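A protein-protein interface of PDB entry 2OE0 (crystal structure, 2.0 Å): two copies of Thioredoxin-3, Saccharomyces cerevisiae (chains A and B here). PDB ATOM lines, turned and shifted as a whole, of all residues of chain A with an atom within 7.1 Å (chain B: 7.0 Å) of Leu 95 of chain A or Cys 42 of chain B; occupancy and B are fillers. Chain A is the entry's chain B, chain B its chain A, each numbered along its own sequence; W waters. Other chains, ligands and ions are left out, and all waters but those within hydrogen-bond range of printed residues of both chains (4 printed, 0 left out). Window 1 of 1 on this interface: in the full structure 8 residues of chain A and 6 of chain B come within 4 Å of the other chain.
The backbone NH of Gly 43 of chain B lies within hydrogen-bond range of the backbone carbonyl oxygen of Leu 95 of chain A, at 2.8 Å.
The side-chain sulfur (SG) of Cys 45 of chain B forms a disulfide with the side-chain sulfur (SG) of Cys 42 of chain B (2.2 Å).
N of Ile 96 of chain A sits at hydrogen-bond distance from O of Leu 89 of chain A (2.7 Å).
The backbone NH of Leu 89 of chain A sits at hydrogen-bond distance from the backbone carbonyl oxygen of Gly 97 of chain A.
Among the printed residues, merely in contact across the chains: Glu 78 of chain A with Trp 41 of chain B (3.4 Å), Cys 79 of chain A with Trp 41 of chain B (3.5 Å), Gln 94 of chain A with Gly 43 of chain B (3.3 Å), Gln 94 of chain A with Pro 44 of chain B (3.5 Å), Leu 95 of chain A with Trp 41 of chain B (3.6 Å), Leu 95 of chain A with Cys 42 of chain B (3.6 Å), Leu 95 of chain A with Pro 44 of chain B (3.5 Å), Ile 96 of chain A with Pro 44 of chain B (3.96 Å) and Gly 97 of chain A with Trp 41 of chain B (3.7 Å).
Of the printed residues of chain B, Cys 79 of chain A touches Trp 41.
Val 88 of chain A touches none of the printed residues of chain B.
Leu 95 of chain A touches four residues of chain B.
Cys 42 of chain B touches just one residue of chain A: Leu 95.
Of the printed residues of chain A, Gly 43 of chain B touches Gln 94 and Leu 95.
The nearest residue of chain B that does not touch Leu 95 of chain A is Cys 45 of chain B (6.3 Å).
The nearest residue of chain A that does not touch Cys 42 of chain B is Ile 96 of chain A (4.7 Å).
Hydrophobic or aromatic side chains of chain A that line the printed part of chain B: Leu 95 and Ile 96.
Of the 15 printed residues of chain B, 4 touch a printed residue of chain A.
Hydrophobic or aromatic side chains of chain B that line the printed part of chain A: Trp 41 and Pro 44.
Along chain B the printed residues that touch a printed residue of chain A span positions 41 to 44.
Among the printed residues, 10 pairs touch across the chains.
Among the printed residues, no Asp or Glu carboxylate lies within 4 Å of a Lys or Arg side-chain nitrogen of the other chain.
1 position is printed for both chains.
Water W3 lies within hydrogen-bond range of the backbone carbonyl oxygen (O) of Ile 96 of chain A and the backbone carbonyl oxygen (O) of Met 84 of chain B.
Water W4 lies within hydrogen-bond range of the backbone carbonyl oxygen of Glu 78 of chain A and the side-chain hydroxyl of Thr 40 of chain B.
Water W2 lies within hydrogen-bond range of O of Ile 96 of chain A (2.7 Å) and N of Met 84 of chain B (2.9 Å).
Water W1 lies within hydrogen-bond range of the backbone NH (N) of Leu 95 of chain A (2.7 Å), the backbone carbonyl oxygen (O) of Trp 41 of chain B (3.4 Å) and the backbone NH (N) of Gly 43 of chain B (3.5 Å).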
ATOM      1  N   PHE A  23      25.196   9.248   1.166  1.00  0.00           N
ATOM      2  CA  PHE A  23      23.721   9.038   1.208  1.00  0.00           C
ATOM      3  C   PHE A  23      23.095   9.438  -0.137  1.00  0.00           C
ATOM      4  O   PHE A  23      22.380   8.656  -0.767  1.00  0.00           O
ATOM      5  CB  PHE A  23      23.187   9.829   2.437  1.00  0.00           C
ATOM      6  CG  PHE A  23      21.693  10.195   2.419  1.00  0.00           C
ATOM      7  CD1 PHE A  23      20.714   9.271   2.752  1.00  0.00           C
ATOM      8  CD2 PHE A  23      21.301  11.503   2.188  1.00  0.00           C
ATOM      9  CE1 PHE A  23      19.339   9.636   2.819  1.00  0.00           C
ATOM     10  CE2 PHE A  23      19.949  11.874   2.237  1.00  0.00           C
ATOM     11  CZ  PHE A  23      18.979  10.925   2.558  1.00  0.00           C
ATOM     12  N   ILE A  27      21.266   6.882  -3.048  1.00  0.00           N
ATOM     13  CA  ILE A  27      19.889   7.108  -3.496  1.00  0.00           C
ATOM     14  C   ILE A  27      19.864   7.097  -5.043  1.00  0.00           C
ATOM     15  O   ILE A  27      19.023   6.453  -5.656  1.00  0.00           O
ATOM     16  CB  ILE A  27      19.309   8.432  -2.939  1.00  0.00           C
ATOM     17  CG1 ILE A  27      19.149   8.387  -1.422  1.00  0.00           C
ATOM     18  CG2 ILE A  27      17.920   8.707  -3.526  1.00  0.00           C
ATOM     19  CD1 ILE A  27      19.145   9.766  -0.762  1.00  0.00           C
ATOM     20  N   LEU A  33      15.680   1.076  -2.508  1.00  0.00           N
ATOM     21  CA  LEU A  33      16.500   1.413  -1.331  1.00  0.00           C
ATOM     22  C   LEU A  33      15.670   1.447  -0.028  1.00  0.00           C
ATOM     23  O   LEU A  33      14.589   2.021   0.007  1.00  0.00           O
ATOM     24  CB  LEU A  33      17.209   2.773  -1.535  1.00  0.00           C
ATOM     25  CG  LEU A  33      18.172   3.253  -0.420  1.00  0.00           C
ATOM     26  CD1 LEU A  33      19.457   2.414  -0.327  1.00  0.00           C
ATOM     27  CD2 LEU A  33      18.548   4.680  -0.627  1.00  0.00           C
ATOM     28  N   ILE A  35      16.380   2.614   4.031  1.00  0.00           N
ATOM     29  CA  ILE A  35      17.311   3.138   5.041  1.00  0.00           C
ATOM     30  C   ILE A  35      16.676   3.025   6.430  1.00  0.00           C
ATOM     31  O   ILE A  35      15.608   3.622   6.681  1.00  0.00           O
ATOM     32  CB  ILE A  35      17.674   4.622   4.782  1.00  0.00           C
ATOM     33  CG1 ILE A  35      18.071   4.852   3.313  1.00  0.00           C
ATOM     34  CG2 ILE A  35      18.792   5.114   5.787  1.00  0.00           C
ATOM     35  CD1 ILE A  35      18.244   6.321   3.006  1.00  0.00           C
ATOM     36  N   PHE A  37      16.890   4.294   9.827  1.00  0.00           N
ATOM     37  CA  PHE A  37      17.362   5.323  10.758  1.00  0.00           C
ATOM     38  C   PHE A  37      17.035   4.903  12.183  1.00  0.00           C
ATOM     39  O   PHE A  37      15.851   4.839  12.574  1.00  0.00           O
ATOM     40  CB  PHE A  37      16.683   6.654  10.461  1.00  0.00           C
ATOM     41  CG  PHE A  37      17.228   7.356   9.255  1.00  0.00           C
ATOM     42  CD1 PHE A  37      16.537   7.309   8.030  1.00  0.00           C
ATOM     43  CD2 PHE A  37      18.394   8.101   9.339  1.00  0.00           C
ATOM     44  CE1 PHE A  37      17.037   7.993   6.904  1.00  0.00           C
ATOM     45  CE2 PHE A  37      18.894   8.762   8.210  1.00  0.00           C
ATOM     46  CZ  PHE A  37      18.223   8.685   7.004  1.00  0.00           C
ATOM     47  N   GLU A  78      18.206  15.718   7.332  1.00  0.00           N
ATOM     48  CA  GLU A  78      17.829  15.755   5.918  1.00  0.00           C
ATOM     49  C   GLU A  78      16.532  14.994   5.644  1.00  0.00           C
ATOM     50  O   GLU A  78      15.714  15.425   4.827  1.00  0.00           O
ATOM     51  CB  GLU A  78      18.972  15.166   5.063  1.00  0.00           C
ATOM     52  CG  GLU A  78      18.691  15.129   3.580  1.00  0.00           C
ATOM     53  CD  GLU A  78      19.126  16.414   2.855  1.00  0.00           C
ATOM     54  OE1 GLU A  78      19.496  17.413   3.515  1.00  0.00           O
ATOM     55  OE2 GLU A  78      19.106  16.404   1.601  1.00  0.00           O
ATOM     56  N   CYS A  79      16.353  13.857   6.323  1.00  0.00           N
ATOM     57  CA  CYS A  79      15.156  13.019   6.199  1.00  0.00           C
ATOM     58  C   CYS A  79      14.077  13.276   7.280  1.00  0.00           C
ATOM     59  O   CYS A  79      13.131  12.482   7.417  1.00  0.00           O
ATOM     60  CB  CYS A  79      15.561  11.543   6.202  1.00  0.00           C
ATOM     61  SG  CYS A  79      16.393  11.077   4.696  1.00  0.00           S
ATOM     62  N   VAL A  88      13.173   4.771   5.587  1.00  0.00           N
ATOM     63  CA  VAL A  88      13.002   5.681   4.465  1.00  0.00           C
ATOM     64  C   VAL A  88      13.164   4.848   3.174  1.00  0.00           C
ATOM     65  O   VAL A  88      14.110   4.049   3.052  1.00  0.00           O
ATOM     66  CB  VAL A  88      13.978   6.882   4.568  1.00  0.00           C
ATOM     67  CG1 VAL A  88      13.928   7.740   3.307  1.00  0.00           C
ATOM     68  CG2 VAL A  88      13.614   7.770   5.795  1.00  0.00           C
ATOM     69  N   LEU A  89      12.197   4.975   2.265  1.00  0.00           N
ATOM     70  CA  LEU A  89      12.191   4.177   1.020  1.00  0.00           C
ATOM     71  C   LEU A  89      12.490   5.051  -0.184  1.00  0.00           C
ATOM     72  O   LEU A  89      11.937   6.155  -0.305  1.00  0.00           O
ATOM     73  CB  LEU A  89      10.858   3.436   0.798  1.00  0.00           C
ATOM     74  CG  LEU A  89      10.212   2.648   1.966  1.00  0.00           C
ATOM     75  CD1 LEU A  89       8.927   1.885   1.543  1.00  0.00           C
ATOM     76  CD2 LEU A  89      11.151   1.707   2.636  1.00  0.00           C
ATOM     77  N   GLY A  90      13.355   4.531  -1.055  1.00  0.00           N
ATOM     78  CA  GLY A  90      13.733   5.168  -2.294  1.00  0.00           C
ATOM     79  C   GLY A  90      13.490   4.239  -3.474  1.00  0.00           C
ATOM     80  O   GLY A  90      13.619   3.009  -3.370  1.00  0.00           O
ATOM     81  N   LYS A  91      13.098   4.832  -4.601  1.00  0.00           N
ATOM     82  CA  LYS A  91      12.797   4.069  -5.787  1.00  0.00           C
ATOM     83  C   LYS A  91      13.297   4.875  -6.989  1.00  0.00           C
ATOM     84  O   LYS A  91      13.021   6.098  -7.078  1.00  0.00           O
ATOM     85  CB  LYS A  91      11.275   3.802  -5.860  1.00  0.00           C
ATOM     86  CG  LYS A  91      10.741   3.319  -7.202  1.00  0.00           C
ATOM     87  CD  LYS A  91      10.667   1.819  -7.300  1.00  0.00           C
ATOM     88  CE  LYS A  91       9.859   1.387  -8.542  1.00  0.00           C
ATOM     89  NZ  LYS A  91       8.373   1.494  -8.276  1.00  0.00           N
ATOM     90  N   ASP A  92      14.049   4.196  -7.869  1.00  0.00           N
ATOM     91  CA  ASP A  92      14.526   4.791  -9.130  1.00  0.00           C
ATOM     92  C   ASP A  92      15.183   6.188  -8.929  1.00  0.00           C
ATOM     93  O   ASP A  92      14.924   7.134  -9.676  1.00  0.00           O
ATOM     94  CB  ASP A  92      13.379   4.860 -10.162  1.00  0.00           C
ATOM     95  CG  ASP A  92      12.872   3.470 -10.597  1.00  0.00           C
ATOM     96  OD1 ASP A  92      13.661   2.503 -10.573  1.00  0.00           O
ATOM     97  OD2 ASP A  92      11.685   3.355 -10.982  1.00  0.00           O
ATOM     98  N   GLY A  93      16.027   6.299  -7.905  1.00  0.00           N
ATOM     99  CA  GLY A  93      16.925   7.424  -7.783  1.00  0.00           C
ATOM    100  C   GLY A  93      16.388   8.560  -6.937  1.00  0.00           C
ATOM    101  O   GLY A  93      16.983   9.662  -6.900  1.00  0.00           O
ATOM    102  N   GLN A  94      15.270   8.316  -6.264  1.00  0.00           N
ATOM    103  CA  GLN A  94      14.712   9.341  -5.382  1.00  0.00           C
ATOM    104  C   GLN A  94      14.018   8.736  -4.165  1.00  0.00           C
ATOM    105  O   GLN A  94      13.537   7.598  -4.201  1.00  0.00           O
ATOM    106  CB  GLN A  94      13.756  10.270  -6.148  1.00  0.00           C
ATOM    107  CG  GLN A  94      12.531   9.558  -6.644  1.00  0.00           C
ATOM    108  CD  GLN A  94      11.635  10.433  -7.496  1.00  0.00           C
ATOM    109  OE1 GLN A  94      11.788  11.655  -7.548  1.00  0.00           O
ATOM    110  NE2 GLN A  94      10.677   9.800  -8.160  1.00  0.00           N
ATOM    111  N   LEU A  95      13.972   9.501  -3.086  1.00  0.00           N
ATOM    112  CA  LEU A  95      13.247   9.057  -1.905  1.00  0.00           C
ATOM    113  C   LEU A  95      11.738   9.279  -2.079  1.00  0.00           C
ATOM    114  O   LEU A  95      11.306  10.385  -2.430  1.00  0.00           O
ATOM    115  CB  LEU A  95      13.745   9.780  -0.650  1.00  0.00           C
ATOM    116  CG  LEU A  95      15.243   9.627  -0.331  1.00  0.00           C
ATOM    117  CD1 LEU A  95      15.541  10.449   0.904  1.00  0.00           C
ATOM    118  CD2 LEU A  95      15.551   8.119  -0.109  1.00  0.00           C
ATOM    119  N   ILE A  96      10.945   8.250  -1.773  1.00  0.00           N
ATOM    120  CA  ILE A  96       9.491   8.307  -2.026  1.00  0.00           C
ATOM    121  C   ILE A  96       8.571   8.214  -0.812  1.00  0.00           C
ATOM    122  O   ILE A  96       7.420   8.671  -0.866  1.00  0.00           O
ATOM    123  CB  ILE A  96       9.057   7.278  -3.096  1.00  0.00           C
ATOM    124  CG1 ILE A  96       9.398   5.846  -2.648  1.00  0.00           C
ATOM    125  CG2 ILE A  96       9.675   7.656  -4.473  1.00  0.00           C
ATOM    126  CD1 ILE A  96       8.671   4.781  -3.390  1.00  0.00           C
ATOM    127  N   GLY A  97       9.052   7.621   0.277  1.00  0.00           N
ATOM    128  CA  GLY A  97       8.188   7.319   1.401  1.00  0.00           C
ATOM    129  C   GLY A  97       8.942   7.060   2.680  1.00  0.00           C
ATOM    130  O   GLY A  97      10.160   6.832   2.666  1.00  0.00           O
ATOM    131  N   PHE B  37       0.277  18.717   0.669  1.00  0.00           N
ATOM    132  CA  PHE B  37       0.950  18.033   1.775  1.00  0.00           C
ATOM    133  C   PHE B  37       2.217  17.362   1.259  1.00  0.00           C
ATOM    134  O   PHE B  37       2.146  16.433   0.441  1.00  0.00           O
ATOM    135  CB  PHE B  37       0.060  16.970   2.439  1.00  0.00           C
ATOM    136  CG  PHE B  37      -1.015  17.546   3.335  1.00  0.00           C
ATOM    137  CD1 PHE B  37      -2.288  17.773   2.850  1.00  0.00           C
ATOM    138  CD2 PHE B  37      -0.746  17.851   4.671  1.00  0.00           C
ATOM    139  CE1 PHE B  37      -3.293  18.295   3.668  1.00  0.00           C
ATOM    140  CE2 PHE B  37      -1.743  18.387   5.486  1.00  0.00           C
ATOM    141  CZ  PHE B  37      -3.026  18.612   4.972  1.00  0.00           C
ATOM    142  N   TYR B  38       3.365  17.820   1.745  1.00  0.00           N
ATOM    143  CA  TYR B  38       4.644  17.385   1.188  1.00  0.00           C
ATOM    144  C   TYR B  38       5.639  17.055   2.270  1.00  0.00           C
ATOM    145  O   TYR B  38       5.390  17.322   3.446  1.00  0.00           O
ATOM    146  CB  TYR B  38       5.267  18.486   0.304  1.00  0.00           C
ATOM    147  CG  TYR B  38       5.693  19.736   1.098  1.00  0.00           C
ATOM    148  CD1 TYR B  38       7.028  19.921   1.510  1.00  0.00           C
ATOM    149  CD2 TYR B  38       4.751  20.688   1.475  1.00  0.00           C
ATOM    150  CE1 TYR B  38       7.410  21.030   2.227  1.00  0.00           C
ATOM    151  CE2 TYR B  38       5.111  21.821   2.243  1.00  0.00           C
ATOM    152  CZ  TYR B  38       6.435  21.990   2.588  1.00  0.00           C
ATOM    153  OH  TYR B  38       6.786  23.104   3.320  1.00  0.00           O
ATOM    154  N   ALA B  39       6.784  16.503   1.840  1.00  0.00           N
ATOM    155  CA  ALA B  39       7.936  16.355   2.722  1.00  0.00           C
ATOM    156  C   ALA B  39       9.174  16.866   1.976  1.00  0.00           C
ATOM    157  O   ALA B  39       9.299  16.676   0.758  1.00  0.00           O
ATOM    158  CB  ALA B  39       8.086  14.905   3.184  1.00  0.00           C
ATOM    159  N   THR B  40      10.080  17.539   2.696  1.00  0.00           N
ATOM    160  CA  THR B  40      11.248  18.194   2.070  1.00  0.00           C
ATOM    161  C   THR B  40      12.236  17.213   1.442  1.00  0.00           C
ATOM    162  O   THR B  40      12.923  17.568   0.501  1.00  0.00           O
ATOM    163  CB  THR B  40      12.027  19.111   3.074  1.00  0.00           C
ATOM    164  OG1 THR B  40      12.338  18.374   4.259  1.00  0.00           O
ATOM    165  CG2 THR B  40      11.201  20.381   3.463  1.00  0.00           C
ATOM    166  N   TRP B  41      12.298  15.985   1.955  1.00  0.00           N
ATOM    167  CA  TRP B  41      13.259  14.958   1.455  1.00  0.00           C
ATOM    168  C   TRP B  41      12.657  14.156   0.271  1.00  0.00           C
ATOM    169  O   TRP B  41      13.344  13.347  -0.347  1.00  0.00           O
ATOM    170  CB  TRP B  41      13.626  13.980   2.602  1.00  0.00           C
ATOM    171  CG  TRP B  41      12.380  13.519   3.394  1.00  0.00           C
ATOM    172  CD1 TRP B  41      11.907  14.043   4.582  1.00  0.00           C
ATOM    173  CD2 TRP B  41      11.435  12.494   3.009  1.00  0.00           C
ATOM    174  NE1 TRP B  41      10.737  13.393   4.955  1.00  0.00           N
ATOM    175  CE2 TRP B  41      10.433  12.441   4.016  1.00  0.00           C
ATOM    176  CE3 TRP B  41      11.339  11.618   1.915  1.00  0.00           C
ATOM    177  CZ2 TRP B  41       9.346  11.554   3.947  1.00  0.00           C
ATOM    178  CZ3 TRP B  41      10.258  10.716   1.867  1.00  0.00           C
ATOM    179  CH2 TRP B  41       9.294  10.694   2.878  1.00  0.00           C
ATOM    180  N   CYS B  42      11.373  14.379  -0.016  1.00  0.00           N
ATOM    181  CA  CYS B  42      10.559  13.520  -0.890  1.00  0.00           C
ATOM    182  C   CYS B  42      10.747  13.959  -2.355  1.00  0.00           C
ATOM    183  O   CYS B  42      10.387  15.078  -2.695  1.00  0.00           O
ATOM    184  CB  CYS B  42       9.083  13.602  -0.423  1.00  0.00           C
ATOM    185  SG  CYS B  42       7.665  13.328  -1.597  1.00  0.00           S
ATOM    186  N   GLY B  43      11.336  13.093  -3.193  1.00  0.00           N
ATOM    187  CA  GLY B  43      11.619  13.417  -4.605  1.00  0.00           C
ATOM    188  C   GLY B  43      10.400  13.807  -5.453  1.00  0.00           C
ATOM    189  O   GLY B  43      10.418  14.811  -6.165  1.00  0.00           O
ATOM    190  N   PRO B  44       9.336  12.994  -5.424  1.00  0.00           N
ATOM    191  CA  PRO B  44       8.085  13.398  -6.099  1.00  0.00           C
ATOM    192  C   PRO B  44       7.505  14.761  -5.679  1.00  0.00           C
ATOM    193  O   PRO B  44       6.918  15.489  -6.516  1.00  0.00           O
ATOM    194  CB  PRO B  44       7.145  12.232  -5.772  1.00  0.00           C
ATOM    195  CG  PRO B  44       8.086  11.063  -5.730  1.00  0.00           C
ATOM    196  CD  PRO B  44       9.220  11.633  -4.884  1.00  0.00           C
ATOM    197  N   CYS B  45       7.689  15.121  -4.409  1.00  0.00           N
ATOM    198  CA  CYS B  45       7.267  16.427  -3.916  1.00  0.00           C
ATOM    199  C   CYS B  45       8.087  17.534  -4.592  1.00  0.00           C
ATOM    200  O   CYS B  45       7.520  18.499  -5.153  1.00  0.00           O
ATOM    201  CB  CYS B  45       7.355  16.466  -2.374  1.00  0.00           C
ATOM    202  SG  CYS B  45       6.395  15.144  -1.548  1.00  0.00           S
ATOM    203  N   LYS B  46       9.412  17.363  -4.595  1.00  0.00           N
ATOM    204  CA  LYS B  46      10.309  18.321  -5.220  1.00  0.00           C
ATOM    205  C   LYS B  46       9.942  18.489  -6.698  1.00  0.00           C
ATOM    206  O   LYS B  46       9.845  19.629  -7.182  1.00  0.00           O
ATOM    207  CB  LYS B  46      11.769  17.873  -5.073  1.00  0.00           C
ATOM    208  CG  LYS B  46      12.316  17.959  -3.668  1.00  0.00           C
ATOM    209  CD  LYS B  46      13.690  17.273  -3.577  1.00  0.00           C
ATOM    210  CE  LYS B  46      14.278  17.463  -2.186  1.00  0.00           C
ATOM    211  NZ  LYS B  46      15.476  16.623  -1.955  1.00  0.00           N
ATOM    212  N   MET B  47       9.710  17.358  -7.387  1.00  0.00           N
ATOM    213  CA  MET B  47       9.299  17.340  -8.804  1.00  0.00           C
ATOM    214  C   MET B  47       8.055  18.194  -9.069  1.00  0.00           C
ATOM    215  O   MET B  47       7.985  18.919 -10.063  1.00  0.00           O
ATOM    216  CB  MET B  47       9.080  15.894  -9.317  1.00  0.00           C
ATOM    217  CG  MET B  47       8.545  15.769 -10.792  1.00  0.00           C
ATOM    218  SD  MET B  47       6.733  15.951 -11.097  1.00  0.00           S
ATOM    219  CE  MET B  47       6.299  14.259 -11.552  1.00  0.00           C
ATOM    220  N   GLN B  49       7.002  20.856  -7.448  1.00  0.00           N
ATOM    221  CA  GLN B  49       7.083  22.300  -7.080  1.00  0.00           C
ATOM    222  C   GLN B  49       6.930  23.297  -8.262  1.00  0.00           C
ATOM    223  O   GLN B  49       6.124  24.216  -8.161  1.00  0.00           O
ATOM    224  CB  GLN B  49       8.318  22.628  -6.228  1.00  0.00           C
ATOM    225  CG  GLN B  49       8.383  21.876  -4.854  1.00  0.00           C
ATOM    226  CD  GLN B  49       9.713  22.100  -4.136  1.00  0.00           C
ATOM    227  OE1 GLN B  49      10.576  22.822  -4.641  1.00  0.00           O
ATOM    228  NE2 GLN B  49       9.894  21.469  -2.961  1.00  0.00           N
ATOM    229  N   ALA B  83       0.401   9.113   1.373  1.00  0.00           N
ATOM    230  CA  ALA B  83       1.343   9.265   0.254  1.00  0.00           C
ATOM    231  C   ALA B  83       1.827  10.726   0.093  1.00  0.00           C
ATOM    232  O   ALA B  83       1.087  11.655   0.428  1.00  0.00           O
ATOM    233  CB  ALA B  83       0.710   8.771  -1.016  1.00  0.00           C
ATOM    234  N   MET B  84       3.058  10.890  -0.417  1.00  0.00           N
ATOM    235  CA  MET B  84       3.718  12.198  -0.612  1.00  0.00           C
ATOM    236  C   MET B  84       3.981  12.408  -2.122  1.00  0.00           C
ATOM    237  O   MET B  84       4.507  11.507  -2.756  1.00  0.00           O
ATOM    238  CB  MET B  84       5.114  12.170   0.027  1.00  0.00           C
ATOM    239  CG  MET B  84       5.258  12.087   1.551  1.00  0.00           C
ATOM    240  SD  MET B  84       4.279  13.353   2.327  1.00  0.00           S
ATOM    241  CE  MET B  84       3.174  12.210   3.092  1.00  0.00           C
ATOM    242  N   PRO B  85       3.597  13.566  -2.710  1.00  0.00           N
ATOM    243  CA  PRO B  85       2.716  14.618  -2.215  1.00  0.00           C
ATOM    244  C   PRO B  85       1.258  14.150  -2.248  1.00  0.00           C
ATOM    245  O   PRO B  85       0.901  13.248  -3.021  1.00  0.00           O
ATOM    246  CB  PRO B  85       2.907  15.745  -3.231  1.00  0.00           C
ATOM    247  CG  PRO B  85       3.205  15.009  -4.533  1.00  0.00           C
ATOM    248  CD  PRO B  85       4.075  13.859  -4.083  1.00  0.00           C
HETATM  249  O   HOH W   1      14.686  12.087  -3.165  1.00  0.00           O
HETATM  250  O   HOH W   2       4.857   8.583  -0.198  1.00  0.00           O
HETATM  251  O   HOH W   3       6.704   9.673  -3.031  1.00  0.00           O
HETATM  252  O   HOH W   4      15.036  17.749   3.947  1.00  0.00           O
